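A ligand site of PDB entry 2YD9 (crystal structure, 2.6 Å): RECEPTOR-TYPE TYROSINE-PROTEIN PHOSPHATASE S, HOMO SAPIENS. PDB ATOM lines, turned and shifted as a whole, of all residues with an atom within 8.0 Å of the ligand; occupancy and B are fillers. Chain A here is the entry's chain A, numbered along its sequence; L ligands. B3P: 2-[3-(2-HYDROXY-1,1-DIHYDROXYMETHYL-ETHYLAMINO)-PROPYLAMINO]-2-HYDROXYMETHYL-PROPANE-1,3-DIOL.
CA of Ala 131 touches O6 of the ligand (3.4 Å). Ile 140 touches the ligand (CD1 to C7, 3.3 Å). Gly 164 touches the ligand. Hydrophobic or aromatic side chains within 4 Å of the ligand: Pro 138 and Ile 140. Nine residues have an atom within 4 Å of the ligand: Cys 130, Ala 131, Ala 132, Asp 137, Pro 138, Ile 140, Arg 162, Ser 163 and Gly 164.
The backbone NH (N) of Ala 165 sits at hydrogen-bond distance from the side-chain hydroxyl (OG) of Ser 163, 3.4 Å away. O of Ile 140 sits at hydrogen-bond distance from NE2 of Gln 160 (2.9 Å). The backbone NH (N) of Asp 112 lies within hydrogen-bond range of the backbone carbonyl oxygen (O) of Ala 131, 2.8 Å away. N of Ala 131 sits at hydrogen-bond distance from O of Met 113. The side-chain sulfur of Cys 130 is disulfide-bonded to the side-chain sulfur of Cys 181 (2.1 Å).
O5 of the ligand lies within hydrogen-bond range of O of Pro 138. O6 of the ligand sits at hydrogen-bond distance from N of Ala 132, 2.9 Å away. N1 of the ligand is in hydrogen-bond range of O of Ala 132, 2.5 Å away. O of Arg 162 is in hydrogen-bond range of O4 of the ligand (2.7 Å). A nitrogen (N2) of the ligand is in salt-bridge range of the side-chain carboxylate (OD1) of Asp 137 (3.5 Å). O4 of the ligand is in hydrogen-bond range of O of Ser 163 (3.0 Å). O6 of the ligand lies within hydrogen-bond range of O of Cys 130 (3.4 Å).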
ATOM      1  N   ASN A 110      -6.159 -21.263 -24.485  1.00  0.00           N
ATOM      2  CA  ASN A 110      -5.464 -22.527 -24.333  1.00  0.00           C
ATOM      3  C   ASN A 110      -3.946 -22.289 -24.349  1.00  0.00           C
ATOM      4  O   ASN A 110      -3.469 -21.457 -25.118  1.00  0.00           O
ATOM      5  CB  ASN A 110      -5.860 -23.469 -25.469  1.00  0.00           C
ATOM      6  CG  ASN A 110      -5.096 -24.758 -25.436  1.00  0.00           C
ATOM      7  OD1 ASN A 110      -5.280 -25.586 -24.534  1.00  0.00           O
ATOM      8  ND2 ASN A 110      -4.214 -24.947 -26.413  1.00  0.00           N
ATOM      9  N   ILE A 111      -3.207 -23.012 -23.522  1.00  0.00           N
ATOM     10  CA  ILE A 111      -1.745 -22.898 -23.509  1.00  0.00           C
ATOM     11  C   ILE A 111      -1.131 -23.933 -24.450  1.00  0.00           C
ATOM     12  O   ILE A 111      -1.104 -25.120 -24.149  1.00  0.00           O
ATOM     13  CB  ILE A 111      -1.164 -23.075 -22.089  1.00  0.00           C
ATOM     14  CG1 ILE A 111      -1.883 -22.183 -21.072  1.00  0.00           C
ATOM     15  CG2 ILE A 111       0.324 -22.739 -22.084  1.00  0.00           C
ATOM     16  CD1 ILE A 111      -1.836 -20.709 -21.390  1.00  0.00           C
ATOM     17  N   ASP A 112      -0.647 -23.480 -25.605  1.00  0.00           N
ATOM     18  CA  ASP A 112      -0.056 -24.360 -26.616  1.00  0.00           C
ATOM     19  C   ASP A 112       1.317 -24.862 -26.184  1.00  0.00           C
ATOM     20  O   ASP A 112       1.630 -26.041 -26.306  1.00  0.00           O
ATOM     21  CB  ASP A 112       0.055 -23.635 -27.961  1.00  0.00           C
ATOM     22  CG  ASP A 112      -1.290 -23.155 -28.478  1.00  0.00           C
ATOM     23  OD1 ASP A 112      -2.220 -23.983 -28.549  1.00  0.00           O
ATOM     24  OD2 ASP A 112      -1.402 -21.943 -28.798  1.00  0.00           O
ATOM     25  N   MET A 113       2.157 -23.946 -25.713  1.00  0.00           N
ATOM     26  CA  MET A 113       3.468 -24.287 -25.152  1.00  0.00           C
ATOM     27  C   MET A 113       3.687 -23.408 -23.941  1.00  0.00           C
ATOM     28  O   MET A 113       3.773 -22.197 -24.076  1.00  0.00           O
ATOM     29  CB  MET A 113       4.579 -24.041 -26.181  1.00  0.00           C
ATOM     30  CG  MET A 113       5.981 -24.403 -25.714  1.00  0.00           C
ATOM     31  SD  MET A 113       7.251 -24.178 -26.976  1.00  0.00           S
ATOM     32  CE  MET A 113       6.631 -25.215 -28.304  1.00  0.00           C
ATOM     33  N   LEU A 129       9.360 -19.182 -22.058  1.00  0.00           N
ATOM     34  CA  LEU A 129       8.459 -19.255 -23.211  1.00  0.00           C
ATOM     35  C   LEU A 129       7.002 -19.397 -22.792  1.00  0.00           C
ATOM     36  O   LEU A 129       6.704 -19.954 -21.755  1.00  0.00           O
ATOM     37  CB  LEU A 129       8.822 -20.443 -24.090  1.00  0.00           C
ATOM     38  CG  LEU A 129      10.196 -20.459 -24.735  1.00  0.00           C
ATOM     39  CD1 LEU A 129      10.262 -21.559 -25.793  1.00  0.00           C
ATOM     40  CD2 LEU A 129      10.536 -19.118 -25.361  1.00  0.00           C
ATOM     41  N   CYS A 130       6.100 -18.887 -23.634  1.00  0.00           N
ATOM     42  CA  CYS A 130       4.671 -19.136 -23.471  1.00  0.00           C
ATOM     43  C   CYS A 130       3.895 -18.782 -24.747  1.00  0.00           C
ATOM     44  O   CYS A 130       3.821 -17.615 -25.130  1.00  0.00           O
ATOM     45  CB  CYS A 130       4.111 -18.401 -22.247  1.00  0.00           C
ATOM     46  SG  CYS A 130       2.337 -18.269 -22.234  1.00  0.00           S
ATOM     47  N   ALA A 131       3.332 -19.801 -25.399  1.00  0.00           N
ATOM     48  CA  ALA A 131       2.498 -19.629 -26.589  1.00  0.00           C
ATOM     49  C   ALA A 131       1.075 -20.056 -26.255  1.00  0.00           C
ATOM     50  O   ALA A 131       0.850 -21.168 -25.776  1.00  0.00           O
ATOM     51  CB  ALA A 131       3.061 -20.446 -27.771  1.00  0.00           C
ATOM     52  N   ALA A 132       0.113 -19.161 -26.508  1.00  0.00           N
ATOM     53  CA  ALA A 132      -1.302 -19.403 -26.185  1.00  0.00           C
ATOM     54  C   ALA A 132      -2.234 -18.971 -27.310  1.00  0.00           C
ATOM     55  O   ALA A 132      -2.029 -17.935 -27.926  1.00  0.00           O
ATOM     56  CB  ALA A 132      -1.670 -18.675 -24.907  1.00  0.00           C
ATOM     57  N   SER A 133      -3.258 -19.767 -27.560  1.00  0.00           N
ATOM     58  CA  SER A 133      -4.275 -19.428 -28.550  1.00  0.00           C
ATOM     59  C   SER A 133      -5.604 -19.138 -27.877  1.00  0.00           C
ATOM     60  O   SER A 133      -5.793 -19.440 -26.702  1.00  0.00           O
ATOM     61  CB  SER A 133      -4.432 -20.593 -29.535  1.00  0.00           C
ATOM     62  OG  SER A 133      -4.533 -21.814 -28.843  1.00  0.00           O
ATOM     63  N   GLY A 134      -6.514 -18.534 -28.638  1.00  0.00           N
ATOM     64  CA  GLY A 134      -7.837 -18.165 -28.144  1.00  0.00           C
ATOM     65  C   GLY A 134      -8.504 -17.246 -29.147  1.00  0.00           C
ATOM     66  O   GLY A 134      -7.889 -16.864 -30.139  1.00  0.00           O
ATOM     67  N   ASN A 135      -9.757 -16.879 -28.893  1.00  0.00           N
ATOM     68  CA  ASN A 135     -10.490 -15.983 -29.789  1.00  0.00           C
ATOM     69  C   ASN A 135     -11.387 -15.025 -29.007  1.00  0.00           C
ATOM     70  O   ASN A 135     -12.427 -15.438 -28.489  1.00  0.00           O
ATOM     71  CB  ASN A 135     -11.306 -16.792 -30.797  1.00  0.00           C
ATOM     72  CG  ASN A 135     -11.835 -15.952 -31.938  1.00  0.00           C
ATOM     73  OD1 ASN A 135     -11.814 -14.714 -31.893  1.00  0.00           O
ATOM     74  ND2 ASN A 135     -12.298 -16.610 -32.997  1.00  0.00           N
ATOM     75  N   PRO A 136     -10.990 -13.739 -28.918  1.00  0.00           N
ATOM     76  CA  PRO A 136      -9.775 -13.124 -29.460  1.00  0.00           C
ATOM     77  C   PRO A 136      -8.477 -13.672 -28.885  1.00  0.00           C
ATOM     78  O   PRO A 136      -8.466 -14.371 -27.862  1.00  0.00           O
ATOM     79  CB  PRO A 136      -9.925 -11.649 -29.058  1.00  0.00           C
ATOM     80  CG  PRO A 136     -11.371 -11.452 -28.892  1.00  0.00           C
ATOM     81  CD  PRO A 136     -11.883 -12.733 -28.308  1.00  0.00           C
ATOM     82  N   ASP A 137      -7.373 -13.356 -29.568  1.00  0.00           N
ATOM     83  CA  ASP A 137      -6.060 -13.785 -29.128  1.00  0.00           C
ATOM     84  C   ASP A 137      -5.863 -13.274 -27.711  1.00  0.00           C
ATOM     85  O   ASP A 137      -6.160 -12.113 -27.435  1.00  0.00           O
ATOM     86  CB  ASP A 137      -4.974 -13.235 -30.059  1.00  0.00           C
ATOM     87  CG  ASP A 137      -4.973 -13.904 -31.422  1.00  0.00           C
ATOM     88  OD1 ASP A 137      -5.759 -14.853 -31.631  1.00  0.00           O
ATOM     89  OD2 ASP A 137      -4.196 -13.480 -32.294  1.00  0.00           O
ATOM     90  N   PRO A 138      -5.387 -14.137 -26.807  1.00  0.00           N
ATOM     91  CA  PRO A 138      -5.284 -13.746 -25.408  1.00  0.00           C
ATOM     92  C   PRO A 138      -4.104 -12.837 -25.115  1.00  0.00           C
ATOM     93  O   PRO A 138      -3.110 -12.835 -25.855  1.00  0.00           O
ATOM     94  CB  PRO A 138      -5.124 -15.083 -24.681  1.00  0.00           C
ATOM     95  CG  PRO A 138      -4.506 -15.976 -25.686  1.00  0.00           C
ATOM     96  CD  PRO A 138      -5.013 -15.541 -27.023  1.00  0.00           C
ATOM     97  N   GLU A 139      -4.229 -12.046 -24.050  1.00  0.00           N
ATOM     98  CA  GLU A 139      -3.173 -11.177 -23.562  1.00  0.00           C
ATOM     99  C   GLU A 139      -2.393 -11.940 -22.514  1.00  0.00           C
ATOM    100  O   GLU A 139      -2.975 -12.401 -21.520  1.00  0.00           O
ATOM    101  CB  GLU A 139      -3.770  -9.920 -22.927  1.00  0.00           C
ATOM    102  CG  GLU A 139      -4.605  -9.044 -23.866  1.00  0.00           C
ATOM    103  CD  GLU A 139      -3.798  -7.929 -24.514  1.00  0.00           C
ATOM    104  OE1 GLU A 139      -3.074  -7.209 -23.776  1.00  0.00           O
ATOM    105  OE2 GLU A 139      -3.895  -7.754 -25.747  1.00  0.00           O
ATOM    106  N   ILE A 140      -1.081 -12.081 -22.699  1.00  0.00           N
ATOM    107  CA  ILE A 140      -0.250 -12.778 -21.717  1.00  0.00           C
ATOM    108  C   ILE A 140       0.189 -11.839 -20.592  1.00  0.00           C
ATOM    109  O   ILE A 140       0.791 -10.800 -20.849  1.00  0.00           O
ATOM    110  CB  ILE A 140       0.996 -13.430 -22.362  1.00  0.00           C
ATOM    111  CG1 ILE A 140       0.647 -14.777 -22.986  1.00  0.00           C
ATOM    112  CG2 ILE A 140       2.061 -13.685 -21.326  1.00  0.00           C
ATOM    113  CD1 ILE A 140      -0.445 -14.729 -24.028  1.00  0.00           C
ATOM    114  N   GLN A 160       8.536  -8.326 -21.790  1.00  0.00           N
ATOM    115  CA  GLN A 160       7.755  -9.325 -22.502  1.00  0.00           C
ATOM    116  C   GLN A 160       7.979  -9.160 -23.993  1.00  0.00           C
ATOM    117  O   GLN A 160       7.984  -8.038 -24.497  1.00  0.00           O
ATOM    118  CB  GLN A 160       6.279  -9.147 -22.186  1.00  0.00           C
ATOM    119  CG  GLN A 160       5.438 -10.354 -22.490  1.00  0.00           C
ATOM    120  CD  GLN A 160       4.075 -10.306 -21.798  1.00  0.00           C
ATOM    121  OE1 GLN A 160       3.992 -10.264 -20.562  1.00  0.00           O
ATOM    122  NE2 GLN A 160       3.007 -10.315 -22.592  1.00  0.00           N
ATOM    123  N   LEU A 161       8.187 -10.270 -24.697  1.00  0.00           N
ATOM    124  CA  LEU A 161       8.374 -10.208 -26.141  1.00  0.00           C
ATOM    125  C   LEU A 161       6.994 -10.274 -26.809  1.00  0.00           C
ATOM    126  O   LEU A 161       6.005 -10.570 -26.157  1.00  0.00           O
ATOM    127  CB  LEU A 161       9.273 -11.372 -26.620  1.00  0.00           C
ATOM    128  CG  LEU A 161      10.540 -11.632 -25.772  1.00  0.00           C
ATOM    129  CD1 LEU A 161      11.408 -12.720 -26.379  1.00  0.00           C
ATOM    130  CD2 LEU A 161      11.336 -10.348 -25.616  1.00  0.00           C
ATOM    131  N   ARG A 162       6.927  -9.984 -28.108  1.00  0.00           N
ATOM    132  CA  ARG A 162       5.658 -10.035 -28.845  1.00  0.00           C
ATOM    133  C   ARG A 162       5.001 -11.414 -28.759  1.00  0.00           C
ATOM    134  O   ARG A 162       3.802 -11.534 -28.889  1.00  0.00           O
ATOM    135  CB  ARG A 162       5.863  -9.721 -30.331  1.00  0.00           C
ATOM    136  CG  ARG A 162       6.390  -8.337 -30.670  1.00  0.00           C
ATOM    137  CD  ARG A 162       7.206  -8.397 -31.970  1.00  0.00           C
ATOM    138  NE  ARG A 162       6.405  -8.893 -33.094  1.00  0.00           N
ATOM    139  CZ  ARG A 162       6.898  -9.431 -34.210  1.00  0.00           C
ATOM    140  NH1 ARG A 162       8.207  -9.562 -34.399  1.00  0.00           N
ATOM    141  NH2 ARG A 162       6.070  -9.831 -35.170  1.00  0.00           N
ATOM    142  N   SER A 163       5.818 -12.447 -28.573  1.00  0.00           N
ATOM    143  CA  SER A 163       5.348 -13.823 -28.556  1.00  0.00           C
ATOM    144  C   SER A 163       4.655 -14.188 -27.248  1.00  0.00           C
ATOM    145  O   SER A 163       3.934 -15.191 -27.196  1.00  0.00           O
ATOM    146  CB  SER A 163       6.507 -14.778 -28.823  1.00  0.00           C
ATOM    147  OG  SER A 163       7.466 -14.727 -27.772  1.00  0.00           O
ATOM    148  N   GLY A 164       4.864 -13.387 -26.214  1.00  0.00           N
ATOM    149  CA  GLY A 164       4.344 -13.685 -24.879  1.00  0.00           C
ATOM    150  C   GLY A 164       5.488 -14.057 -23.949  1.00  0.00           C
ATOM    151  O   GLY A 164       5.352 -13.989 -22.726  1.00  0.00           O
ATOM    152  N   ALA A 165       6.620 -14.441 -24.527  1.00  0.00           N
ATOM    153  CA  ALA A 165       7.808 -14.814 -23.784  1.00  0.00           C
ATOM    154  C   ALA A 165       8.214 -13.736 -22.765  1.00  0.00           C
ATOM    155  O   ALA A 165       8.249 -12.559 -23.110  1.00  0.00           O
ATOM    156  CB  ALA A 165       8.960 -15.084 -24.727  1.00  0.00           C
ATOM    157  N   CYS A 181       2.690 -18.576 -16.747  1.00  0.00           N
ATOM    158  CA  CYS A 181       2.133 -17.595 -17.688  1.00  0.00           C
ATOM    159  C   CYS A 181       0.607 -17.713 -17.667  1.00  0.00           C
ATOM    160  O   CYS A 181       0.054 -18.806 -17.534  1.00  0.00           O
ATOM    161  CB  CYS A 181       2.698 -17.749 -19.126  1.00  0.00           C
ATOM    162  SG  CYS A 181       1.680 -18.680 -20.296  1.00  0.00           S
ATOM    163  N   VAL A 182      -0.061 -16.571 -17.813  1.00  0.00           N
ATOM    164  CA  VAL A 182      -1.509 -16.484 -17.766  1.00  0.00           C
ATOM    165  C   VAL A 182      -2.030 -15.844 -19.038  1.00  0.00           C
ATOM    166  O   VAL A 182      -1.560 -14.766 -19.426  1.00  0.00           O
ATOM    167  CB  VAL A 182      -1.968 -15.623 -16.569  1.00  0.00           C
ATOM    168  CG1 VAL A 182      -3.486 -15.534 -16.528  1.00  0.00           C
ATOM    169  CG2 VAL A 182      -1.405 -16.190 -15.277  1.00  0.00           C
ATOM    170  N   ALA A 183      -2.994 -16.504 -19.681  1.00  0.00           N
ATOM    171  CA  ALA A 183      -3.615 -15.977 -20.892  1.00  0.00           C
ATOM    172  C   ALA A 183      -5.041 -15.542 -20.565  1.00  0.00           C
ATOM    173  O   ALA A 183      -5.805 -16.307 -19.978  1.00  0.00           O
ATOM    174  CB  ALA A 183      -3.632 -17.028 -21.997  1.00  0.00           C
ATOM    175  N   THR A 184      -5.373 -14.302 -20.925  1.00  0.00           N
ATOM    176  CA  THR A 184      -6.684 -13.746 -20.650  1.00  0.00           C
ATOM    177  C   THR A 184      -7.288 -13.161 -21.923  1.00  0.00           C
ATOM    178  O   THR A 184      -6.598 -12.476 -22.678  1.00  0.00           O
ATOM    179  CB  THR A 184      -6.611 -12.642 -19.560  1.00  0.00           C
ATOM    180  OG1 THR A 184      -6.141 -13.193 -18.337  1.00  0.00           O
ATOM    181  CG2 THR A 184      -7.968 -11.998 -19.342  1.00  0.00           C
ATOM    182  N   ASN A 185      -8.565 -13.434 -22.148  1.00  0.00           N
ATOM    183  CA  ASN A 185      -9.351 -12.718 -23.142  1.00  0.00           C
ATOM    184  C   ASN A 185     -10.813 -12.603 -22.675  1.00  0.00           C
ATOM    185  O   ASN A 185     -11.088 -12.842 -21.503  1.00  0.00           O
ATOM    186  CB  ASN A 185      -9.195 -13.364 -24.525  1.00  0.00           C
ATOM    187  CG  ASN A 185      -9.927 -14.679 -24.661  1.00  0.00           C
ATOM    188  OD1 ASN A 185     -10.645 -15.117 -23.751  1.00  0.00           O
ATOM    189  ND2 ASN A 185      -9.762 -15.327 -25.815  1.00  0.00           N
HETATM  190  C1  B3P L   1      -1.870 -17.179 -30.942  1.00  0.00           C
HETATM  191  C2  B3P L   1      -1.974 -17.125 -32.471  1.00  0.00           C
HETATM  192  C3  B3P L   1      -1.352 -15.879 -30.328  1.00  0.00           C
HETATM  193  N1  B3P L   1      -0.622 -16.201 -29.085  1.00  0.00           N
HETATM  194  C4  B3P L   1       0.068 -15.018 -28.523  1.00  0.00           C
HETATM  195  C5  B3P L   1       1.303 -14.722 -29.384  1.00  0.00           C
HETATM  196  C6  B3P L   1      -0.879 -13.805 -28.481  1.00  0.00           C
HETATM  197  C7  B3P L   1       0.513 -15.312 -27.086  1.00  0.00           C
HETATM  198  N2  B3P L   1      -3.385 -17.159 -32.906  1.00  0.00           N
HETATM  199  C8  B3P L   1      -3.454 -17.344 -34.364  1.00  0.00           C
HETATM  200  C9  B3P L   1      -2.056 -17.402 -35.021  1.00  0.00           C
HETATM  201  C10 B3P L   1      -4.199 -16.147 -34.966  1.00  0.00           C
HETATM  202  C11 B3P L   1      -4.256 -18.616 -34.667  1.00  0.00           C
HETATM  203  O1  B3P L   1      -1.454 -18.699 -34.893  1.00  0.00           O
HETATM  204  O2  B3P L   1      -5.383 -15.874 -34.206  1.00  0.00           O
HETATM  205  O3  B3P L   1      -4.104 -18.955 -36.046  1.00  0.00           O
HETATM  206  O4  B3P L   1       2.034 -13.628 -28.827  1.00  0.00           O
HETATM  207  O5  B3P L   1      -2.058 -14.127 -27.734  1.00  0.00           O
HETATM  208  O6  B3P L   1       1.259 -16.530 -27.056  1.00  0.00           O
